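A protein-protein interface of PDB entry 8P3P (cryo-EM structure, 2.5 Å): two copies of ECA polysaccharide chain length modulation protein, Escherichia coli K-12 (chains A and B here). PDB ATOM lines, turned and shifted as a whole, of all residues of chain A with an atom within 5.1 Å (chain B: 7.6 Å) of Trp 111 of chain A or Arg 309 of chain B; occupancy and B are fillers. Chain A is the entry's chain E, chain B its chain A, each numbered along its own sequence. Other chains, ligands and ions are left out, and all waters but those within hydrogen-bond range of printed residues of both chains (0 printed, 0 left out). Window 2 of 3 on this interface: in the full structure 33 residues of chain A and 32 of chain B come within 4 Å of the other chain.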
ATOM      1  N   ALA A 109     -19.995   3.347  -2.499  1.00  0.00           N
ATOM      2  CA  ALA A 109     -20.782   3.551  -1.290  1.00  0.00           C
ATOM      3  C   ALA A 109     -20.060   4.374  -0.233  1.00  0.00           C
ATOM      4  O   ALA A 109     -20.673   4.712   0.785  1.00  0.00           O
ATOM      5  CB  ALA A 109     -21.190   2.200  -0.697  1.00  0.00           C
ATOM      6  N   SER A 110     -18.791   4.707  -0.442  1.00  0.00           N
ATOM      7  CA  SER A 110     -18.005   5.362   0.595  1.00  0.00           C
ATOM      8  C   SER A 110     -18.436   6.812   0.785  1.00  0.00           C
ATOM      9  O   SER A 110     -18.622   7.554  -0.180  1.00  0.00           O
ATOM     10  CB  SER A 110     -16.520   5.302   0.246  1.00  0.00           C
ATOM     11  OG  SER A 110     -15.742   5.989   1.208  1.00  0.00           O
ATOM     12  N   TRP A 111     -18.587   7.210   2.051  1.00  0.00           N
ATOM     13  CA  TRP A 111     -18.898   8.599   2.372  1.00  0.00           C
ATOM     14  C   TRP A 111     -17.769   9.527   1.942  1.00  0.00           C
ATOM     15  O   TRP A 111     -18.014  10.632   1.442  1.00  0.00           O
ATOM     16  CB  TRP A 111     -19.164   8.726   3.874  1.00  0.00           C
ATOM     17  CG  TRP A 111     -19.352  10.127   4.381  1.00  0.00           C
ATOM     18  CD1 TRP A 111     -18.381  11.060   4.605  1.00  0.00           C
ATOM     19  CD2 TRP A 111     -20.588  10.738   4.763  1.00  0.00           C
ATOM     20  NE1 TRP A 111     -18.938  12.218   5.085  1.00  0.00           N
ATOM     21  CE2 TRP A 111     -20.293  12.045   5.192  1.00  0.00           C
ATOM     22  CE3 TRP A 111     -21.917  10.308   4.776  1.00  0.00           C
ATOM     23  CZ2 TRP A 111     -21.277  12.926   5.628  1.00  0.00           C
ATOM     24  CZ3 TRP A 111     -22.892  11.183   5.209  1.00  0.00           C
ATOM     25  CH2 TRP A 111     -22.568  12.477   5.630  1.00  0.00           C
ATOM     26  N   ASP A 112     -16.522   9.093   2.138  1.00  0.00           N
ATOM     27  CA  ASP A 112     -15.377   9.921   1.778  1.00  0.00           C
ATOM     28  C   ASP A 112     -15.343  10.195   0.282  1.00  0.00           C
ATOM     29  O   ASP A 112     -15.013  11.307  -0.144  1.00  0.00           O
ATOM     30  CB  ASP A 112     -14.086   9.243   2.227  1.00  0.00           C
ATOM     31  CG  ASP A 112     -13.792   9.465   3.694  1.00  0.00           C
ATOM     32  OD1 ASP A 112     -14.657  10.026   4.397  1.00  0.00           O
ATOM     33  OD2 ASP A 112     -12.697   9.075   4.147  1.00  0.00           O
ATOM     34  N   THR A 113     -15.665   9.188  -0.531  1.00  0.00           N
ATOM     35  CA  THR A 113     -15.669   9.376  -1.977  1.00  0.00           C
ATOM     36  C   THR A 113     -16.668  10.450  -2.384  1.00  0.00           C
ATOM     37  O   THR A 113     -16.351  11.336  -3.185  1.00  0.00           O
ATOM     38  CB  THR A 113     -15.990   8.057  -2.678  1.00  0.00           C
ATOM     39  OG1 THR A 113     -15.136   7.024  -2.173  1.00  0.00           O
ATOM     40  CG2 THR A 113     -15.783   8.187  -4.176  1.00  0.00           C
ATOM     41  N   ARG A 114     -17.881  10.390  -1.832  1.00  0.00           N
ATOM     42  CA  ARG A 114     -18.883  11.404  -2.139  1.00  0.00           C
ATOM     43  C   ARG A 114     -18.435  12.778  -1.665  1.00  0.00           C
ATOM     44  O   ARG A 114     -18.641  13.780  -2.360  1.00  0.00           O
ATOM     45  CB  ARG A 114     -20.222  11.029  -1.510  1.00  0.00           C
ATOM     46  CG  ARG A 114     -20.549   9.554  -1.604  1.00  0.00           C
ATOM     47  CD  ARG A 114     -22.028   9.294  -1.413  1.00  0.00           C
ATOM     48  NE  ARG A 114     -22.424   9.371  -0.013  1.00  0.00           N
ATOM     49  CZ  ARG A 114     -22.562   8.320   0.784  1.00  0.00           C
ATOM     50  NH1 ARG A 114     -22.330   7.092   0.353  1.00  0.00           N
ATOM     51  NH2 ARG A 114     -22.942   8.507   2.043  1.00  0.00           N
ATOM     52  N   ARG A 115     -17.812  12.846  -0.486  1.00  0.00           N
ATOM     53  CA  ARG A 115     -17.344  14.132   0.024  1.00  0.00           C
ATOM     54  C   ARG A 115     -16.319  14.758  -0.913  1.00  0.00           C
ATOM     55  O   ARG A 115     -16.451  15.925  -1.303  1.00  0.00           O
ATOM     56  CB  ARG A 115     -16.758  13.963   1.424  1.00  0.00           C
ATOM     57  CG  ARG A 115     -16.430  15.281   2.095  1.00  0.00           C
ATOM     58  CD  ARG A 115     -16.021  15.091   3.540  1.00  0.00           C
ATOM     59  NE  ARG A 115     -15.866  16.369   4.221  1.00  0.00           N
ATOM     60  CZ  ARG A 115     -14.787  17.136   4.136  1.00  0.00           C
ATOM     61  NH1 ARG A 115     -13.740  16.778   3.412  1.00  0.00           N
ATOM     62  NH2 ARG A 115     -14.759  18.291   4.794  1.00  0.00           N
ATOM     63  N   ASP A 140     -22.774  18.512   3.520  1.00  0.00           N
ATOM     64  CA  ASP A 140     -23.390  17.349   4.150  1.00  0.00           C
ATOM     65  C   ASP A 140     -24.712  16.998   3.482  1.00  0.00           C
ATOM     66  O   ASP A 140     -25.036  15.818   3.309  1.00  0.00           O
ATOM     67  CB  ASP A 140     -23.592  17.604   5.641  1.00  0.00           C
ATOM     68  CG  ASP A 140     -23.982  16.353   6.398  1.00  0.00           C
ATOM     69  OD1 ASP A 140     -25.186  16.028   6.432  1.00  0.00           O
ATOM     70  OD2 ASP A 140     -23.083  15.692   6.958  1.00  0.00           O
ATOM     71  N   ILE A 143     -23.922  15.331   0.132  1.00  0.00           N
ATOM     72  CA  ILE A 143     -23.355  13.993   0.271  1.00  0.00           C
ATOM     73  C   ILE A 143     -24.468  12.957   0.349  1.00  0.00           C
ATOM     74  O   ILE A 143     -24.382  11.883  -0.259  1.00  0.00           O
ATOM     75  CB  ILE A 143     -22.426  13.924   1.497  1.00  0.00           C
ATOM     76  CG1 ILE A 143     -21.109  14.641   1.209  1.00  0.00           C
ATOM     77  CG2 ILE A 143     -22.152  12.484   1.884  1.00  0.00           C
ATOM     78  CD1 ILE A 143     -20.224  14.787   2.421  1.00  0.00           C
ATOM     79  N   ASN A 144     -25.534  13.267   1.086  1.00  0.00           N
ATOM     80  CA  ASN A 144     -26.678  12.370   1.180  1.00  0.00           C
ATOM     81  C   ASN A 144     -27.485  12.306  -0.109  1.00  0.00           C
ATOM     82  O   ASN A 144     -28.348  11.431  -0.232  1.00  0.00           O
ATOM     83  CB  ASN A 144     -27.584  12.802   2.332  1.00  0.00           C
ATOM     84  CG  ASN A 144     -26.920  12.645   3.682  1.00  0.00           C
ATOM     85  OD1 ASN A 144     -26.679  13.625   4.386  1.00  0.00           O
ATOM     86  ND2 ASN A 144     -26.618  11.407   4.052  1.00  0.00           N
ATOM     87  N   SER B  56     -21.933  14.817  18.129  1.00  0.00           N
ATOM     88  CA  SER B  56     -21.578  13.451  17.769  1.00  0.00           C
ATOM     89  C   SER B  56     -20.829  13.416  16.444  1.00  0.00           C
ATOM     90  O   SER B  56     -21.107  14.196  15.533  1.00  0.00           O
ATOM     91  CB  SER B  56     -22.822  12.565  17.674  1.00  0.00           C
ATOM     92  OG  SER B  56     -22.492  11.277  17.196  1.00  0.00           O
ATOM     93  N   SER B  57     -19.881  12.486  16.347  1.00  0.00           N
ATOM     94  CA  SER B  57     -19.110  12.263  15.133  1.00  0.00           C
ATOM     95  C   SER B  57     -19.036  10.769  14.850  1.00  0.00           C
ATOM     96  O   SER B  57     -19.086   9.948  15.768  1.00  0.00           O
ATOM     97  CB  SER B  57     -17.701  12.847  15.245  1.00  0.00           C
ATOM     98  OG  SER B  57     -16.917  12.493  14.122  1.00  0.00           O
ATOM     99  N   THR B  58     -18.910  10.424  13.570  1.00  0.00           N
ATOM    100  CA  THR B  58     -18.984   9.038  13.125  1.00  0.00           C
ATOM    101  C   THR B  58     -17.806   8.712  12.218  1.00  0.00           C
ATOM    102  O   THR B  58     -17.350   9.561  11.448  1.00  0.00           O
ATOM    103  CB  THR B  58     -20.299   8.770  12.380  1.00  0.00           C
ATOM    104  OG1 THR B  58     -21.394   9.294  13.139  1.00  0.00           O
ATOM    105  CG2 THR B  58     -20.509   7.279  12.175  1.00  0.00           C
ATOM    106  N   ALA B  59     -17.317   7.477  12.320  1.00  0.00           N
ATOM    107  CA  ALA B  59     -16.261   6.967  11.458  1.00  0.00           C
ATOM    108  C   ALA B  59     -16.611   5.556  11.018  1.00  0.00           C
ATOM    109  O   ALA B  59     -17.200   4.788  11.782  1.00  0.00           O
ATOM    110  CB  ALA B  59     -14.906   6.965  12.168  1.00  0.00           C
ATOM    111  N   ILE B  60     -16.253   5.220   9.781  1.00  0.00           N
ATOM    112  CA  ILE B  60     -16.470   3.886   9.234  1.00  0.00           C
ATOM    113  C   ILE B  60     -15.150   3.376   8.682  1.00  0.00           C
ATOM    114  O   ILE B  60     -14.506   4.061   7.881  1.00  0.00           O
ATOM    115  CB  ILE B  60     -17.553   3.878   8.138  1.00  0.00           C
ATOM    116  CG1 ILE B  60     -18.855   4.480   8.666  1.00  0.00           C
ATOM    117  CG2 ILE B  60     -17.787   2.466   7.636  1.00  0.00           C
ATOM    118  CD1 ILE B  60     -20.031   4.295   7.740  1.00  0.00           C
ATOM    119  N   THR B  61     -14.762   2.172   9.090  1.00  0.00           N
ATOM    120  CA  THR B  61     -13.451   1.616   8.788  1.00  0.00           C
ATOM    121  C   THR B  61     -13.585   0.310   8.016  1.00  0.00           C
ATOM    122  O   THR B  61     -14.672  -0.256   7.877  1.00  0.00           O
ATOM    123  CB  THR B  61     -12.647   1.383  10.073  1.00  0.00           C
ATOM    124  OG1 THR B  61     -13.394   0.538  10.954  1.00  0.00           O
ATOM    125  CG2 THR B  61     -12.365   2.703  10.768  1.00  0.00           C
ATOM    126  N   ASP B  62     -12.449  -0.166   7.510  1.00  0.00           N
ATOM    127  CA  ASP B  62     -12.379  -1.423   6.778  1.00  0.00           C
ATOM    128  C   ASP B  62     -10.976  -1.996   6.945  1.00  0.00           C
ATOM    129  O   ASP B  62     -10.127  -1.420   7.630  1.00  0.00           O
ATOM    130  CB  ASP B  62     -12.738  -1.223   5.303  1.00  0.00           C
ATOM    131  CG  ASP B  62     -13.147  -2.514   4.623  1.00  0.00           C
ATOM    132  OD1 ASP B  62     -13.933  -3.279   5.219  1.00  0.00           O
ATOM    133  OD2 ASP B  62     -12.680  -2.765   3.494  1.00  0.00           O
ATOM    134  N   ASP B 159     -18.240  -1.914   9.822  1.00  0.00           N
ATOM    135  CA  ASP B 159     -18.109  -1.532  11.219  1.00  0.00           C
ATOM    136  C   ASP B 159     -18.005  -0.019  11.344  1.00  0.00           C
ATOM    137  O   ASP B 159     -17.315   0.639  10.561  1.00  0.00           O
ATOM    138  CB  ASP B 159     -16.879  -2.193  11.838  1.00  0.00           C
ATOM    139  CG  ASP B 159     -16.814  -3.678  11.558  1.00  0.00           C
ATOM    140  OD1 ASP B 159     -17.874  -4.337  11.595  1.00  0.00           O
ATOM    141  OD2 ASP B 159     -15.706  -4.188  11.299  1.00  0.00           O
ATOM    142  N   SER B 160     -18.698   0.536  12.334  1.00  0.00           N
ATOM    143  CA  SER B 160     -18.703   1.973  12.550  1.00  0.00           C
ATOM    144  C   SER B 160     -18.436   2.276  14.016  1.00  0.00           C
ATOM    145  O   SER B 160     -18.687   1.450  14.895  1.00  0.00           O
ATOM    146  CB  SER B 160     -20.032   2.602  12.117  1.00  0.00           C
ATOM    147  OG  SER B 160     -21.072   2.259  13.013  1.00  0.00           O
ATOM    148  N   VAL B 161     -17.906   3.469  14.269  1.00  0.00           N
ATOM    149  CA  VAL B 161     -17.649   3.942  15.621  1.00  0.00           C
ATOM    150  C   VAL B 161     -18.157   5.372  15.736  1.00  0.00           C
ATOM    151  O   VAL B 161     -17.901   6.202  14.858  1.00  0.00           O
ATOM    152  CB  VAL B 161     -16.153   3.850  15.987  1.00  0.00           C
ATOM    153  CG1 VAL B 161     -15.291   4.499  14.917  1.00  0.00           C
ATOM    154  CG2 VAL B 161     -15.893   4.474  17.347  1.00  0.00           C
ATOM    155  N   LEU B 175     -12.516  11.689  18.065  1.00  0.00           N
ATOM    156  CA  LEU B 175     -12.745  10.458  17.317  1.00  0.00           C
ATOM    157  C   LEU B 175     -11.528  10.088  16.478  1.00  0.00           C
ATOM    158  O   LEU B 175     -11.137   8.913  16.429  1.00  0.00           O
ATOM    159  CB  LEU B 175     -13.983  10.589  16.434  1.00  0.00           C
ATOM    160  CG  LEU B 175     -14.426   9.279  15.777  1.00  0.00           C
ATOM    161  CD1 LEU B 175     -14.451   8.149  16.787  1.00  0.00           C
ATOM    162  CD2 LEU B 175     -15.782   9.439  15.123  1.00  0.00           C
ATOM    163  N   VAL B 179      -9.385   6.620  17.101  1.00  0.00           N
ATOM    164  CA  VAL B 179      -9.130   5.625  16.062  1.00  0.00           C
ATOM    165  C   VAL B 179      -7.633   5.386  15.917  1.00  0.00           C
ATOM    166  O   VAL B 179      -7.181   4.240  15.800  1.00  0.00           O
ATOM    167  CB  VAL B 179      -9.776   6.054  14.734  1.00  0.00           C
ATOM    168  CG1 VAL B 179      -9.363   5.114  13.621  1.00  0.00           C
ATOM    169  CG2 VAL B 179     -11.285   6.071  14.870  1.00  0.00           C
ATOM    170  N   ARG B 306      -8.363   1.038   7.401  1.00  0.00           N
ATOM    171  CA  ARG B 306      -8.483   2.078   6.394  1.00  0.00           C
ATOM    172  C   ARG B 306      -9.851   2.730   6.531  1.00  0.00           C
ATOM    173  O   ARG B 306     -10.822   2.091   6.942  1.00  0.00           O
ATOM    174  CB  ARG B 306      -8.269   1.532   4.977  1.00  0.00           C
ATOM    175  CG  ARG B 306      -9.487   0.921   4.321  1.00  0.00           C
ATOM    176  CD  ARG B 306      -9.131   0.436   2.931  1.00  0.00           C
ATOM    177  NE  ARG B 306     -10.284  -0.070   2.200  1.00  0.00           N
ATOM    178  CZ  ARG B 306     -10.541   0.212   0.931  1.00  0.00           C
ATOM    179  NH1 ARG B 306      -9.751   1.004   0.227  1.00  0.00           N
ATOM    180  NH2 ARG B 306     -11.617  -0.316   0.355  1.00  0.00           N
ATOM    181  N   TYR B 307      -9.913   4.012   6.193  1.00  0.00           N
ATOM    182  CA  TYR B 307     -11.110   4.815   6.401  1.00  0.00           C
ATOM    183  C   TYR B 307     -12.046   4.680   5.207  1.00  0.00           C
ATOM    184  O   TYR B 307     -11.665   4.988   4.074  1.00  0.00           O
ATOM    185  CB  TYR B 307     -10.744   6.282   6.613  1.00  0.00           C
ATOM    186  CG  TYR B 307     -10.590   6.690   8.056  1.00  0.00           C
ATOM    187  CD1 TYR B 307     -11.474   6.242   9.025  1.00  0.00           C
ATOM    188  CD2 TYR B 307      -9.562   7.533   8.449  1.00  0.00           C
ATOM    189  CE1 TYR B 307     -11.336   6.618  10.342  1.00  0.00           C
ATOM    190  CE2 TYR B 307      -9.418   7.916   9.762  1.00  0.00           C
ATOM    191  CZ  TYR B 307     -10.305   7.456  10.704  1.00  0.00           C
ATOM    192  OH  TYR B 307     -10.158   7.839  12.015  1.00  0.00           O
ATOM    193  N   LEU B 308     -13.267   4.217   5.464  1.00  0.00           N
ATOM    194  CA  LEU B 308     -14.341   4.341   4.488  1.00  0.00           C
ATOM    195  C   LEU B 308     -15.147   5.611   4.702  1.00  0.00           C
ATOM    196  O   LEU B 308     -15.721   6.144   3.747  1.00  0.00           O
ATOM    197  CB  LEU B 308     -15.263   3.123   4.553  1.00  0.00           C
ATOM    198  CG  LEU B 308     -14.689   1.836   3.964  1.00  0.00           C
ATOM    199  CD1 LEU B 308     -15.753   0.760   3.904  1.00  0.00           C
ATOM    200  CD2 LEU B 308     -14.112   2.098   2.587  1.00  0.00           C
ATOM    201  N   ARG B 309     -15.194   6.099   5.939  1.00  0.00           N
ATOM    202  CA  ARG B 309     -15.777   7.397   6.263  1.00  0.00           C
ATOM    203  C   ARG B 309     -14.931   8.009   7.368  1.00  0.00           C
ATOM    204  O   ARG B 309     -14.951   7.520   8.502  1.00  0.00           O
ATOM    205  CB  ARG B 309     -17.234   7.274   6.703  1.00  0.00           C
ATOM    206  CG  ARG B 309     -17.771   8.546   7.330  1.00  0.00           C
ATOM    207  CD  ARG B 309     -19.215   8.408   7.757  1.00  0.00           C
ATOM    208  NE  ARG B 309     -19.726   9.659   8.302  1.00  0.00           N
ATOM    209  CZ  ARG B 309     -21.005   9.901   8.550  1.00  0.00           C
ATOM    210  NH1 ARG B 309     -21.937   8.994   8.316  1.00  0.00           N
ATOM    211  NH2 ARG B 309     -21.356  11.083   9.045  1.00  0.00           N
ATOM    212  N   THR B 310     -14.183   9.053   7.028  1.00  0.00           N
ATOM    213  CA  THR B 310     -13.348   9.742   7.998  1.00  0.00           C
ATOM    214  C   THR B 310     -14.214  10.609   8.910  1.00  0.00           C
ATOM    215  O   THR B 310     -15.222  11.165   8.462  1.00  0.00           O
ATOM    216  CB  THR B 310     -12.316  10.608   7.269  1.00  0.00           C
ATOM    217  OG1 THR B 310     -11.674   9.828   6.253  1.00  0.00           O
ATOM    218  CG2 THR B 310     -11.259  11.137   8.219  1.00  0.00           C
ATOM    219  N   PRO B 311     -13.865  10.729  10.193  1.00  0.00           N
ATOM    220  CA  PRO B 311     -14.615  11.632  11.073  1.00  0.00           C
ATOM    221  C   PRO B 311     -14.578  13.068  10.575  1.00  0.00           C
ATOM    222  O   PRO B 311     -13.567  13.540  10.052  1.00  0.00           O
ATOM    223  CB  PRO B 311     -13.899  11.489  12.419  1.00  0.00           C
ATOM    224  CG  PRO B 311     -13.290  10.147  12.377  1.00  0.00           C
ATOM    225  CD  PRO B 311     -12.928   9.879  10.946  1.00  0.00           C
ATOM    226  N   GLU B 312     -15.700  13.763  10.747  1.00  0.00           N
ATOM    227  CA  GLU B 312     -15.823  15.161  10.369  1.00  0.00           C
ATOM    228  C   GLU B 312     -16.607  15.895  11.447  1.00  0.00           C
ATOM    229  O   GLU B 312     -17.287  15.281  12.273  1.00  0.00           O
ATOM    230  CB  GLU B 312     -16.515  15.328   9.009  1.00  0.00           C
ATOM    231  CG  GLU B 312     -15.658  14.947   7.813  1.00  0.00           C
ATOM    232  CD  GLU B 312     -14.363  15.731   7.740  1.00  0.00           C
ATOM    233  OE1 GLU B 312     -14.360  16.921   8.121  1.00  0.00           O
ATOM    234  OE2 GLU B 312     -13.346  15.158   7.296  1.00  0.00           O
ATOM    235  N   PRO B 314     -19.549  17.585  13.109  1.00  0.00           N
ATOM    236  CA  PRO B 314     -20.995  17.526  12.883  1.00  0.00           C
ATOM    237  C   PRO B 314     -21.563  18.896  12.554  1.00  0.00           C
ATOM    238  O   PRO B 314     -21.056  19.929  12.996  1.00  0.00           O
ATOM    239  CB  PRO B 314     -21.543  16.998  14.214  1.00  0.00           C
ATOM    240  CG  PRO B 314     -20.487  17.324  15.214  1.00  0.00           C
ATOM    241  CD  PRO B 314     -19.187  17.209  14.486  1.00  0.00           C
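No position is printed for both chains.
OG of Ser 110 of chain A lies close to N of Asp 112 of chain A, 3.3 Å away. The backbone NH (N) of Arg 309 of chain B sits at hydrogen-bond distance from the backbone carbonyl oxygen (O) of Ile 60 of chain B, at 2.9 Å. The backbone carbonyl oxygen of Ile 60 of chain B sits at hydrogen-bond distance from the backbone NH of Leu 308 of chain B, at 2.7 Å. O of Glu 312 of chain B is in hydrogen-bond range of OG of Ser 57 of chain B (3.4 Å).
Of the 20 printed residues of chain B, 4 touch a printed residue of chain A. Printed residues of chain B that touch a printed residue of chain A: Leu 308, Arg 309, Thr 310 and Glu 312. Hydrophobic or aromatic side chains of chain A that line the printed part of chain B: Trp 111. Along chain A the printed residues that touch a printed residue of chain B span positions 110 to 115.
Printed residues of chain B within 4 Å of Ser 110 of chain A: Leu 308 (2.5 Å). Of chain B, only Leu 308 and Arg 309 come within 4 Å of Trp 111 of chain A. Printed residues of chain B within 4 Å of Asp 112 of chain A: Leu 308 (3.5 Å), Arg 309 (3.4 Å) and Thr 310 (2.5 Å). Printed residues of chain A within 4 Å of Leu 308 of chain B: Ser 110, Trp 111 and Asp 112. Arg 309 of chain B touches just these residues of chain A: Trp 111 (3.7 Å) and Asp 112 (3.4 Å). The nearest residue of chain B that does not touch Trp 111 of chain A is Thr 310 of chain B (5.0 Å). The nearest residue of chain A that does not touch Arg 309 of chain B is Ser 110 of chain A (4.8 Å).
Among the printed residues, merely in contact across the chains: Trp 111 of chain A with Arg 309 of chain B and Asp 112 of chain A with Arg 309 of chain B.
The guanidinium group (NH2) of Arg 115 of chain A is in salt-bridge range of the side-chain carboxylate (OE1) of Glu 312 of chain B (3.6 Å). O of Leu 308 of chain B lies within hydrogen-bond range of OG of Ser 110 of chain A (2.5 Å). The backbone carbonyl oxygen (O) of Leu 308 of chain B lies within hydrogen-bond range of the backbone NH (N) of Asp 112 of chain A. N of Trp 111 of chain A sits at hydrogen-bond distance from O of Leu 308 of chain B. OG1 of Thr 310 of chain B sits at hydrogen-bond distance from OD2 of Asp 112 of chain A, 2.5 Å away.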
